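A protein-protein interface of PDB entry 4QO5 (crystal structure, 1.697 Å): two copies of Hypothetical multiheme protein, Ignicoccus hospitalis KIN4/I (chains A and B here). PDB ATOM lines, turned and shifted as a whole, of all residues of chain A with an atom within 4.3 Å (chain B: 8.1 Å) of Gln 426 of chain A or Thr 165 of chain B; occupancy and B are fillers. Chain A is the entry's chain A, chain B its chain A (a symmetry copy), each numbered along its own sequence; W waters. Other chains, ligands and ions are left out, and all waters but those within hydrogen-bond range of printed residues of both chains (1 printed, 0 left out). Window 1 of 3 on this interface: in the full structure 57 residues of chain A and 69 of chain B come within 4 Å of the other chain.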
ATOM      1  N   LEU A 422      14.642 -24.334  32.935  1.00  0.00           N
ATOM      2  CA  LEU A 422      15.570 -23.817  31.938  1.00  0.00           C
ATOM      3  C   LEU A 422      16.211 -24.992  31.199  1.00  0.00           C
ATOM      4  O   LEU A 422      16.349 -24.972  29.972  1.00  0.00           O
ATOM      5  CB  LEU A 422      16.652 -22.957  32.599  1.00  0.00           C
ATOM      6  CG  LEU A 422      17.626 -22.311  31.625  1.00  0.00           C
ATOM      7  CD1 LEU A 422      16.861 -21.381  30.683  1.00  0.00           C
ATOM      8  CD2 LEU A 422      18.711 -21.560  32.389  1.00  0.00           C
ATOM      9  N   LEU A 423      16.567 -26.030  31.946  1.00  0.00           N
ATOM     10  CA  LEU A 423      17.144 -27.227  31.319  1.00  0.00           C
ATOM     11  C   LEU A 423      16.172 -27.841  30.303  1.00  0.00           C
ATOM     12  O   LEU A 423      16.583 -28.182  29.187  1.00  0.00           O
ATOM     13  CB  LEU A 423      17.584 -28.251  32.365  1.00  0.00           C
ATOM     14  CG  LEU A 423      18.114 -29.607  31.854  1.00  0.00           C
ATOM     15  CD1 LEU A 423      19.381 -29.412  31.025  1.00  0.00           C
ATOM     16  CD2 LEU A 423      18.385 -30.553  33.012  1.00  0.00           C
ATOM     17  N   ASP A 424      14.886 -27.963  30.664  1.00  0.00           N
ATOM     18  CA  ASP A 424      13.899 -28.415  29.685  1.00  0.00           C
ATOM     19  C   ASP A 424      13.889 -27.599  28.389  1.00  0.00           C
ATOM     20  O   ASP A 424      13.765 -28.168  27.303  1.00  0.00           O
ATOM     21  CB  ASP A 424      12.484 -28.431  30.276  1.00  0.00           C
ATOM     22  CG  ASP A 424      12.297 -29.514  31.317  1.00  0.00           C
ATOM     23  OD1 ASP A 424      13.096 -30.482  31.325  1.00  0.00           O
ATOM     24  OD2 ASP A 424      11.345 -29.395  32.122  1.00  0.00           O
ATOM     25  N   THR A 425      13.992 -26.272  28.493  1.00  0.00           N
ATOM     26  CA  THR A 425      13.970 -25.438  27.290  1.00  0.00           C
ATOM     27  C   THR A 425      15.210 -25.695  26.435  1.00  0.00           C
ATOM     28  O   THR A 425      15.146 -25.669  25.201  1.00  0.00           O
ATOM     29  CB  THR A 425      13.850 -23.916  27.591  1.00  0.00           C
ATOM     30  OG1 THR A 425      15.107 -23.398  28.054  1.00  0.00           O
ATOM     31  CG2 THR A 425      12.735 -23.635  28.615  1.00  0.00           C
ATOM     32  N   GLN A 426      16.334 -25.959  27.091  1.00  0.00           N
ATOM     33  CA  GLN A 426      17.569 -26.243  26.356  1.00  0.00           C
ATOM     34  C   GLN A 426      17.572 -27.611  25.691  1.00  0.00           C
ATOM     35  O   GLN A 426      18.145 -27.780  24.611  1.00  0.00           O
ATOM     36  CB  GLN A 426      18.794 -26.046  27.252  1.00  0.00           C
ATOM     37  CG  GLN A 426      18.924 -24.596  27.662  1.00  0.00           C
ATOM     38  CD  GLN A 426      18.832 -23.668  26.465  1.00  0.00           C
ATOM     39  OE1 GLN A 426      19.778 -23.557  25.675  1.00  0.00           O
ATOM     40  NE2 GLN A 426      17.684 -23.006  26.311  1.00  0.00           N
ATOM     41  N   ILE A 427      16.897 -28.569  26.324  1.00  0.00           N
ATOM     42  CA  ILE A 427      16.686 -29.893  25.737  1.00  0.00           C
ATOM     43  C   ILE A 427      15.869 -29.723  24.464  1.00  0.00           C
ATOM     44  O   ILE A 427      16.217 -30.266  23.420  1.00  0.00           O
ATOM     45  CB  ILE A 427      15.977 -30.839  26.737  1.00  0.00           C
ATOM     46  CG1 ILE A 427      16.970 -31.270  27.824  1.00  0.00           C
ATOM     47  CG2 ILE A 427      15.370 -32.071  26.028  1.00  0.00           C
ATOM     48  CD1 ILE A 427      16.315 -31.840  29.064  1.00  0.00           C
ATOM     49  N   GLU A 428      14.797 -28.934  24.548  1.00  0.00           N
ATOM     50  CA  GLU A 428      13.943 -28.662  23.397  1.00  0.00           C
ATOM     51  C   GLU A 428      14.705 -27.961  22.274  1.00  0.00           C
ATOM     52  O   GLU A 428      14.597 -28.336  21.107  1.00  0.00           O
ATOM     53  CB  GLU A 428      12.749 -27.793  23.805  1.00  0.00           C
ATOM     54  CG  GLU A 428      12.000 -27.234  22.600  1.00  0.00           C
ATOM     55  CD  GLU A 428      11.246 -25.953  22.907  1.00  0.00           C
ATOM     56  OE1 GLU A 428      10.431 -25.958  23.855  1.00  0.00           O
ATOM     57  OE2 GLU A 428      11.475 -24.941  22.203  1.00  0.00           O
ATOM     58  N   GLU A 429      15.450 -26.919  22.623  1.00  0.00           N
ATOM     59  CA  GLU A 429      16.167 -26.141  21.611  1.00  0.00           C
ATOM     60  C   GLU A 429      17.331 -26.914  20.990  1.00  0.00           C
ATOM     61  O   GLU A 429      17.500 -26.916  19.769  1.00  0.00           O
ATOM     62  CB  GLU A 429      16.599 -24.785  22.173  1.00  0.00           C
ATOM     63  CG  GLU A 429      15.370 -23.911  22.429  1.00  0.00           C
ATOM     64  CD  GLU A 429      15.667 -22.605  23.132  1.00  0.00           C
ATOM     65  OE1 GLU A 429      16.845 -22.354  23.474  1.00  0.00           O
ATOM     66  OE2 GLU A 429      14.703 -21.831  23.349  1.00  0.00           O
ATOM     67  N   THR A 430      18.117 -27.597  21.807  1.00  0.00           N
ATOM     68  CA  THR A 430      19.224 -28.368  21.237  1.00  0.00           C
ATOM     69  C   THR A 430      18.715 -29.509  20.371  1.00  0.00           C
ATOM     70  O   THR A 430      19.316 -29.819  19.336  1.00  0.00           O
ATOM     71  CB  THR A 430      20.201 -28.913  22.298  1.00  0.00           C
ATOM     72  OG1 THR A 430      19.475 -29.655  23.283  1.00  0.00           O
ATOM     73  CG2 THR A 430      20.961 -27.755  22.957  1.00  0.00           C
ATOM     74  N   ILE A 480      25.817 -28.008  25.748  1.00  0.00           N
ATOM     75  CA  ILE A 480      24.796 -27.022  26.116  1.00  0.00           C
ATOM     76  C   ILE A 480      23.880 -27.559  27.209  1.00  0.00           C
ATOM     77  O   ILE A 480      23.563 -26.864  28.181  1.00  0.00           O
ATOM     78  CB  ILE A 480      23.962 -26.606  24.885  1.00  0.00           C
ATOM     79  CG1 ILE A 480      24.829 -25.784  23.932  1.00  0.00           C
ATOM     80  CG2 ILE A 480      22.725 -25.777  25.309  1.00  0.00           C
ATOM     81  CD1 ILE A 480      24.260 -25.683  22.524  1.00  0.00           C
ATOM     82  N   THR A 484      23.834 -26.317  31.150  1.00  0.00           N
ATOM     83  CA  THR A 484      22.568 -25.811  31.714  1.00  0.00           C
ATOM     84  C   THR A 484      22.238 -26.602  32.974  1.00  0.00           C
ATOM     85  O   THR A 484      21.933 -26.029  34.005  1.00  0.00           O
ATOM     86  CB  THR A 484      21.439 -25.919  30.695  1.00  0.00           C
ATOM     87  OG1 THR A 484      21.826 -25.228  29.501  1.00  0.00           O
ATOM     88  CG2 THR A 484      20.130 -25.313  31.244  1.00  0.00           C
ATOM     89  N   THR A 492      28.437 -23.625  27.571  1.00  0.00           N
ATOM     90  CA  THR A 492      27.174 -23.424  26.873  1.00  0.00           C
ATOM     91  C   THR A 492      27.307 -22.382  25.763  1.00  0.00           C
ATOM     92  O   THR A 492      26.344 -22.116  25.042  1.00  0.00           O
ATOM     93  CB  THR A 492      26.059 -22.928  27.824  1.00  0.00           C
ATOM     94  OG1 THR A 492      26.442 -21.665  28.382  1.00  0.00           O
ATOM     95  CG2 THR A 492      25.834 -23.914  28.949  1.00  0.00           C
ATOM     96  N   TRP A 498      26.487 -22.892  22.347  1.00  0.00           N
ATOM     97  CA  TRP A 498      25.610 -22.328  21.321  1.00  0.00           C
ATOM     98  C   TRP A 498      26.349 -21.751  20.128  1.00  0.00           C
ATOM     99  O   TRP A 498      25.923 -21.925  18.985  1.00  0.00           O
ATOM    100  CB  TRP A 498      24.636 -21.280  21.903  1.00  0.00           C
ATOM    101  CG  TRP A 498      23.410 -21.932  22.461  1.00  0.00           C
ATOM    102  CD1 TRP A 498      23.042 -22.012  23.775  1.00  0.00           C
ATOM    103  CD2 TRP A 498      22.417 -22.646  21.722  1.00  0.00           C
ATOM    104  NE1 TRP A 498      21.865 -22.714  23.894  1.00  0.00           N
ATOM    105  CE2 TRP A 498      21.470 -23.123  22.646  1.00  0.00           C
ATOM    106  CE3 TRP A 498      22.241 -22.936  20.363  1.00  0.00           C
ATOM    107  CZ2 TRP A 498      20.358 -23.880  22.261  1.00  0.00           C
ATOM    108  CZ3 TRP A 498      21.127 -23.684  19.982  1.00  0.00           C
ATOM    109  CH2 TRP A 498      20.205 -24.142  20.926  1.00  0.00           C
ATOM    110  N   THR B 147      23.003 -17.614  19.049  1.00  0.00           N
ATOM    111  CA  THR B 147      22.125 -18.322  19.975  1.00  0.00           C
ATOM    112  C   THR B 147      20.723 -18.558  19.441  1.00  0.00           C
ATOM    113  O   THR B 147      19.846 -19.011  20.174  1.00  0.00           O
ATOM    114  CB  THR B 147      21.977 -17.539  21.286  1.00  0.00           C
ATOM    115  OG1 THR B 147      21.428 -16.246  20.990  1.00  0.00           O
ATOM    116  CG2 THR B 147      23.328 -17.372  21.975  1.00  0.00           C
ATOM    117  N   GLY B 157      15.424 -20.185  20.252  1.00  0.00           N
ATOM    118  CA  GLY B 157      16.407 -19.450  21.017  1.00  0.00           C
ATOM    119  C   GLY B 157      15.932 -18.037  21.294  1.00  0.00           C
ATOM    120  O   GLY B 157      15.043 -17.521  20.616  1.00  0.00           O
ATOM    121  N   GLY B 158      16.516 -17.403  22.301  1.00  0.00           N
ATOM    122  CA  GLY B 158      16.124 -16.047  22.645  1.00  0.00           C
ATOM    123  C   GLY B 158      16.503 -15.700  24.062  1.00  0.00           C
ATOM    124  O   GLY B 158      17.187 -16.464  24.726  1.00  0.00           O
ATOM    125  N   GLU B 159      16.048 -14.541  24.531  1.00  0.00           N
ATOM    126  CA  GLU B 159      16.589 -13.979  25.766  1.00  0.00           C
ATOM    127  C   GLU B 159      16.357 -14.815  27.015  1.00  0.00           C
ATOM    128  O   GLU B 159      17.224 -14.879  27.898  1.00  0.00           O
ATOM    129  CB  GLU B 159      16.057 -12.555  26.001  1.00  0.00           C
ATOM    130  CG  GLU B 159      16.761 -11.865  27.174  1.00  0.00           C
ATOM    131  CD  GLU B 159      16.521 -10.373  27.226  1.00  0.00           C
ATOM    132  OE1 GLU B 159      15.927  -9.826  26.271  1.00  0.00           O
ATOM    133  OE2 GLU B 159      16.924  -9.750  28.231  1.00  0.00           O
ATOM    134  N   ARG B 160      15.188 -15.447  27.095  1.00  0.00           N
ATOM    135  CA  ARG B 160      14.821 -16.192  28.291  1.00  0.00           C
ATOM    136  C   ARG B 160      15.278 -17.654  28.244  1.00  0.00           C
ATOM    137  O   ARG B 160      15.121 -18.390  29.223  1.00  0.00           O
ATOM    138  CB  ARG B 160      13.305 -16.128  28.504  1.00  0.00           C
ATOM    139  N   THR B 161      15.832 -18.085  27.114  1.00  0.00           N
ATOM    140  CA  THR B 161      16.245 -19.487  26.982  1.00  0.00           C
ATOM    141  C   THR B 161      17.720 -19.641  26.606  1.00  0.00           C
ATOM    142  O   THR B 161      18.580 -19.669  27.479  1.00  0.00           O
ATOM    143  CB  THR B 161      15.344 -20.289  26.015  1.00  0.00           C
ATOM    144  OG1 THR B 161      15.327 -19.670  24.716  1.00  0.00           O
ATOM    145  CG2 THR B 161      13.914 -20.375  26.564  1.00  0.00           C
ATOM    146  N   SER B 162      18.011 -19.752  25.319  1.00  0.00           N
ATOM    147  CA  SER B 162      19.406 -19.950  24.895  1.00  0.00           C
ATOM    148  C   SER B 162      20.353 -18.852  25.370  1.00  0.00           C
ATOM    149  O   SER B 162      21.507 -19.126  25.713  1.00  0.00           O
ATOM    150  CB  SER B 162      19.497 -20.102  23.377  1.00  0.00           C
ATOM    151  OG  SER B 162      19.047 -18.926  22.730  1.00  0.00           O
ATOM    152  N   GLN B 163      19.868 -17.611  25.422  1.00  0.00           N
ATOM    153  CA  GLN B 163      20.744 -16.516  25.788  1.00  0.00           C
ATOM    154  C   GLN B 163      20.929 -16.479  27.302  1.00  0.00           C
ATOM    155  O   GLN B 163      21.967 -16.055  27.800  1.00  0.00           O
ATOM    156  CB  GLN B 163      20.221 -15.192  25.212  1.00  0.00           C
ATOM    157  CG  GLN B 163      20.273 -15.211  23.687  1.00  0.00           C
ATOM    158  CD  GLN B 163      19.492 -14.108  23.017  1.00  0.00           C
ATOM    159  OE1 GLN B 163      18.983 -13.189  23.670  1.00  0.00           O
ATOM    160  NE2 GLN B 163      19.388 -14.189  21.694  1.00  0.00           N
ATOM    161  N   GLU B 164      19.924 -16.949  28.029  1.00  0.00           N
ATOM    162  CA  GLU B 164      19.991 -16.942  29.489  1.00  0.00           C
ATOM    163  C   GLU B 164      21.006 -17.940  30.024  1.00  0.00           C
ATOM    164  O   GLU B 164      21.672 -17.693  31.041  1.00  0.00           O
ATOM    165  CB  GLU B 164      18.599 -17.194  30.099  1.00  0.00           C
ATOM    166  CG  GLU B 164      18.631 -17.236  31.615  1.00  0.00           C
ATOM    167  CD  GLU B 164      17.259 -17.057  32.234  1.00  0.00           C
ATOM    168  OE1 GLU B 164      16.936 -17.834  33.153  1.00  0.00           O
ATOM    169  OE2 GLU B 164      16.516 -16.142  31.810  1.00  0.00           O
ATOM    170  N   THR B 165      21.138 -19.069  29.335  1.00  0.00           N
ATOM    171  CA  THR B 165      22.071 -20.096  29.760  1.00  0.00           C
ATOM    172  C   THR B 165      23.466 -19.839  29.198  1.00  0.00           C
ATOM    173  O   THR B 165      24.425 -20.495  29.619  1.00  0.00           O
ATOM    174  CB  THR B 165      21.591 -21.497  29.357  1.00  0.00           C
ATOM    175  OG1 THR B 165      22.261 -22.470  30.161  1.00  0.00           O
ATOM    176  CG2 THR B 165      21.868 -21.773  27.880  1.00  0.00           C
ATOM    177  N   SER B 166      23.569 -18.894  28.258  1.00  0.00           N
ATOM    178  CA  SER B 166      24.867 -18.571  27.639  1.00  0.00           C
ATOM    179  C   SER B 166      25.378 -17.169  27.987  1.00  0.00           C
ATOM    180  O   SER B 166      25.850 -16.955  29.105  1.00  0.00           O
ATOM    181  CB  SER B 166      24.854 -18.818  26.120  1.00  0.00           C
ATOM    182  OG  SER B 166      23.839 -18.110  25.452  1.00  0.00           O
ATOM    183  N   CYS B 167      25.254 -16.221  27.067  1.00  0.00           N
ATOM    184  CA  CYS B 167      25.830 -14.876  27.291  1.00  0.00           C
ATOM    185  C   CYS B 167      25.393 -14.273  28.616  1.00  0.00           C
ATOM    186  O   CYS B 167      26.205 -13.695  29.327  1.00  0.00           O
ATOM    187  CB  CYS B 167      25.447 -13.876  26.214  1.00  0.00           C
ATOM    188  SG  CYS B 167      25.223 -14.471  24.560  1.00  0.00           S
ATOM    189  N   LEU B 168      24.103 -14.388  28.949  1.00  0.00           N
ATOM    190  CA  LEU B 168      23.603 -13.668  30.117  1.00  0.00           C
ATOM    191  C   LEU B 168      24.024 -14.291  31.446  1.00  0.00           C
ATOM    192  O   LEU B 168      23.928 -13.650  32.488  1.00  0.00           O
ATOM    193  CB  LEU B 168      22.083 -13.480  30.034  1.00  0.00           C
ATOM    194  CG  LEU B 168      21.678 -12.848  28.702  1.00  0.00           C
ATOM    195  CD1 LEU B 168      20.179 -12.601  28.673  1.00  0.00           C
ATOM    196  CD2 LEU B 168      22.433 -11.528  28.462  1.00  0.00           C
ATOM    197  N   ALA B 169      24.506 -15.534  31.418  1.00  0.00           N
ATOM    198  CA  ALA B 169      25.041 -16.146  32.634  1.00  0.00           C
ATOM    199  C   ALA B 169      26.250 -15.362  33.170  1.00  0.00           C
ATOM    200  O   ALA B 169      26.474 -15.272  34.381  1.00  0.00           O
ATOM    201  CB  ALA B 169      25.434 -17.607  32.379  1.00  0.00           C
ATOM    202  N   CYS B 170      27.053 -14.810  32.271  1.00  0.00           N
ATOM    203  CA  CYS B 170      28.193 -14.023  32.720  1.00  0.00           C
ATOM    204  C   CYS B 170      27.913 -12.548  32.762  1.00  0.00           C
ATOM    205  O   CYS B 170      28.364 -11.870  33.680  1.00  0.00           O
ATOM    206  CB  CYS B 170      29.380 -14.239  31.812  1.00  0.00           C
ATOM    207  SG  CYS B 170      29.791 -15.997  31.894  1.00  0.00           S
ATOM    208  N   THR B 173      21.312 -10.988  33.643  1.00  0.00           N
ATOM    209  CA  THR B 173      19.971 -10.969  33.079  1.00  0.00           C
ATOM    210  C   THR B 173      19.221  -9.760  33.620  1.00  0.00           C
ATOM    211  O   THR B 173      19.705  -9.057  34.504  1.00  0.00           O
ATOM    212  CB  THR B 173      19.150 -12.199  33.535  1.00  0.00           C
ATOM    213  OG1 THR B 173      19.243 -12.305  34.969  1.00  0.00           O
ATOM    214  CG2 THR B 173      19.657 -13.479  32.891  1.00  0.00           C
ATOM    215  N   ASN B 200      20.406 -15.870  38.660  1.00  0.00           N
ATOM    216  CA  ASN B 200      21.429 -15.394  37.747  1.00  0.00           C
ATOM    217  C   ASN B 200      22.367 -14.572  38.588  1.00  0.00           C
ATOM    218  O   ASN B 200      21.911 -13.857  39.478  1.00  0.00           O
ATOM    219  CB  ASN B 200      20.846 -14.487  36.665  1.00  0.00           C
ATOM    220  CG  ASN B 200      21.930 -13.830  35.825  1.00  0.00           C
ATOM    221  OD1 ASN B 200      22.388 -12.718  36.129  1.00  0.00           O
ATOM    222  ND2 ASN B 200      22.362 -14.521  34.784  1.00  0.00           N
HETATM  223  O   HOH W   1      13.052 -21.226  21.550  1.00  0.00           O
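O of Leu 422 of chain A lies within hydrogen-bond range of OG1 of Thr 425 of chain A (2.8 Å).
The side-chain hydroxyl (OG1) of Thr 425 of chain A is in hydrogen-bond range of the side-chain amide nitrogen (NE2) of Gln 426 of chain A, 3.1 Å away.
OG1 of Thr 430 of chain A lies within hydrogen-bond range of O of Gln 426 of chain A (2.7 Å).
O of Ile 480 of chain A sits at hydrogen-bond distance from OG1 of Thr 484 of chain A, 2.7 Å away.
The backbone NH (N) of Trp 498 of chain A sits at hydrogen-bond distance from the backbone carbonyl oxygen (O) of Thr 492 of chain A, at 2.8 Å.
The backbone carbonyl oxygen (O) of Ser 162 of chain B is in hydrogen-bond range of the side-chain hydroxyl (OG) of Ser 166 of chain B.
NE2 of Gln 426 of chain A sits close to N of Ser 162 of chain B.
The side-chain carboxylate of Glu 429 of chain A lies within hydrogen-bond range of the side-chain hydroxyl of Thr 161 of chain B (2.6 Å).
The backbone NH of Ser 162 of chain B lies within hydrogen-bond range of the side-chain carboxylate of Glu 429 of chain A, 3.4 Å away.
The side-chain hydroxyl of Thr 484 of chain A lies within hydrogen-bond range of the side-chain hydroxyl of Thr 165 of chain B (2.9 Å).
OG1 of Thr 492 of chain A lies within hydrogen-bond range of O of Thr 165 of chain B.
Of the printed residues of chain A, Ser 162 of chain B touches Gln 426, Glu 429 and Trp 498.
Printed residues of chain A within 4 Å of Ser 166 of chain B: Thr 492.
O of Arg 160 of chain B touches CD1 of Leu 422 of chain A, at 3.8 Å.
CG2 of Thr 161 of chain B touches OG1 of Thr 425 of chain A, at 3.6 Å.
Gln 426 of chain A touches Thr 161 of chain B (NE2 to C, 3.4 Å).
OE1 of Gln 426 of chain A touches CG2 of Thr 165 of chain B, 3.5 Å away.
Gly 157 of chain B touches Glu 429 of chain A (N to OE2, 3.6 Å).
Thr 492 of chain A touches Ser 166 of chain B.
NE1 of Trp 498 of chain A touches CB of Ser 162 of chain B, at 3.6 Å.
No position is printed for both chains.
Water W1 lies within hydrogen-bond range of OE2 of Glu 429 of chain A (2.5 Å) and N of Gly 157 of chain B (2.9 Å).
Of the 17 printed residues of chain B, 6 touch a printed residue of chain A.
Printed residues of chain A that touch a printed residue of chain B: Leu 422, Thr 425, Gln 426, Glu 429, Thr 484, Thr 492 and Trp 498.
Hydrophobic or aromatic side chains of chain A that line the printed part of chain B: Leu 422 and Trp 498.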
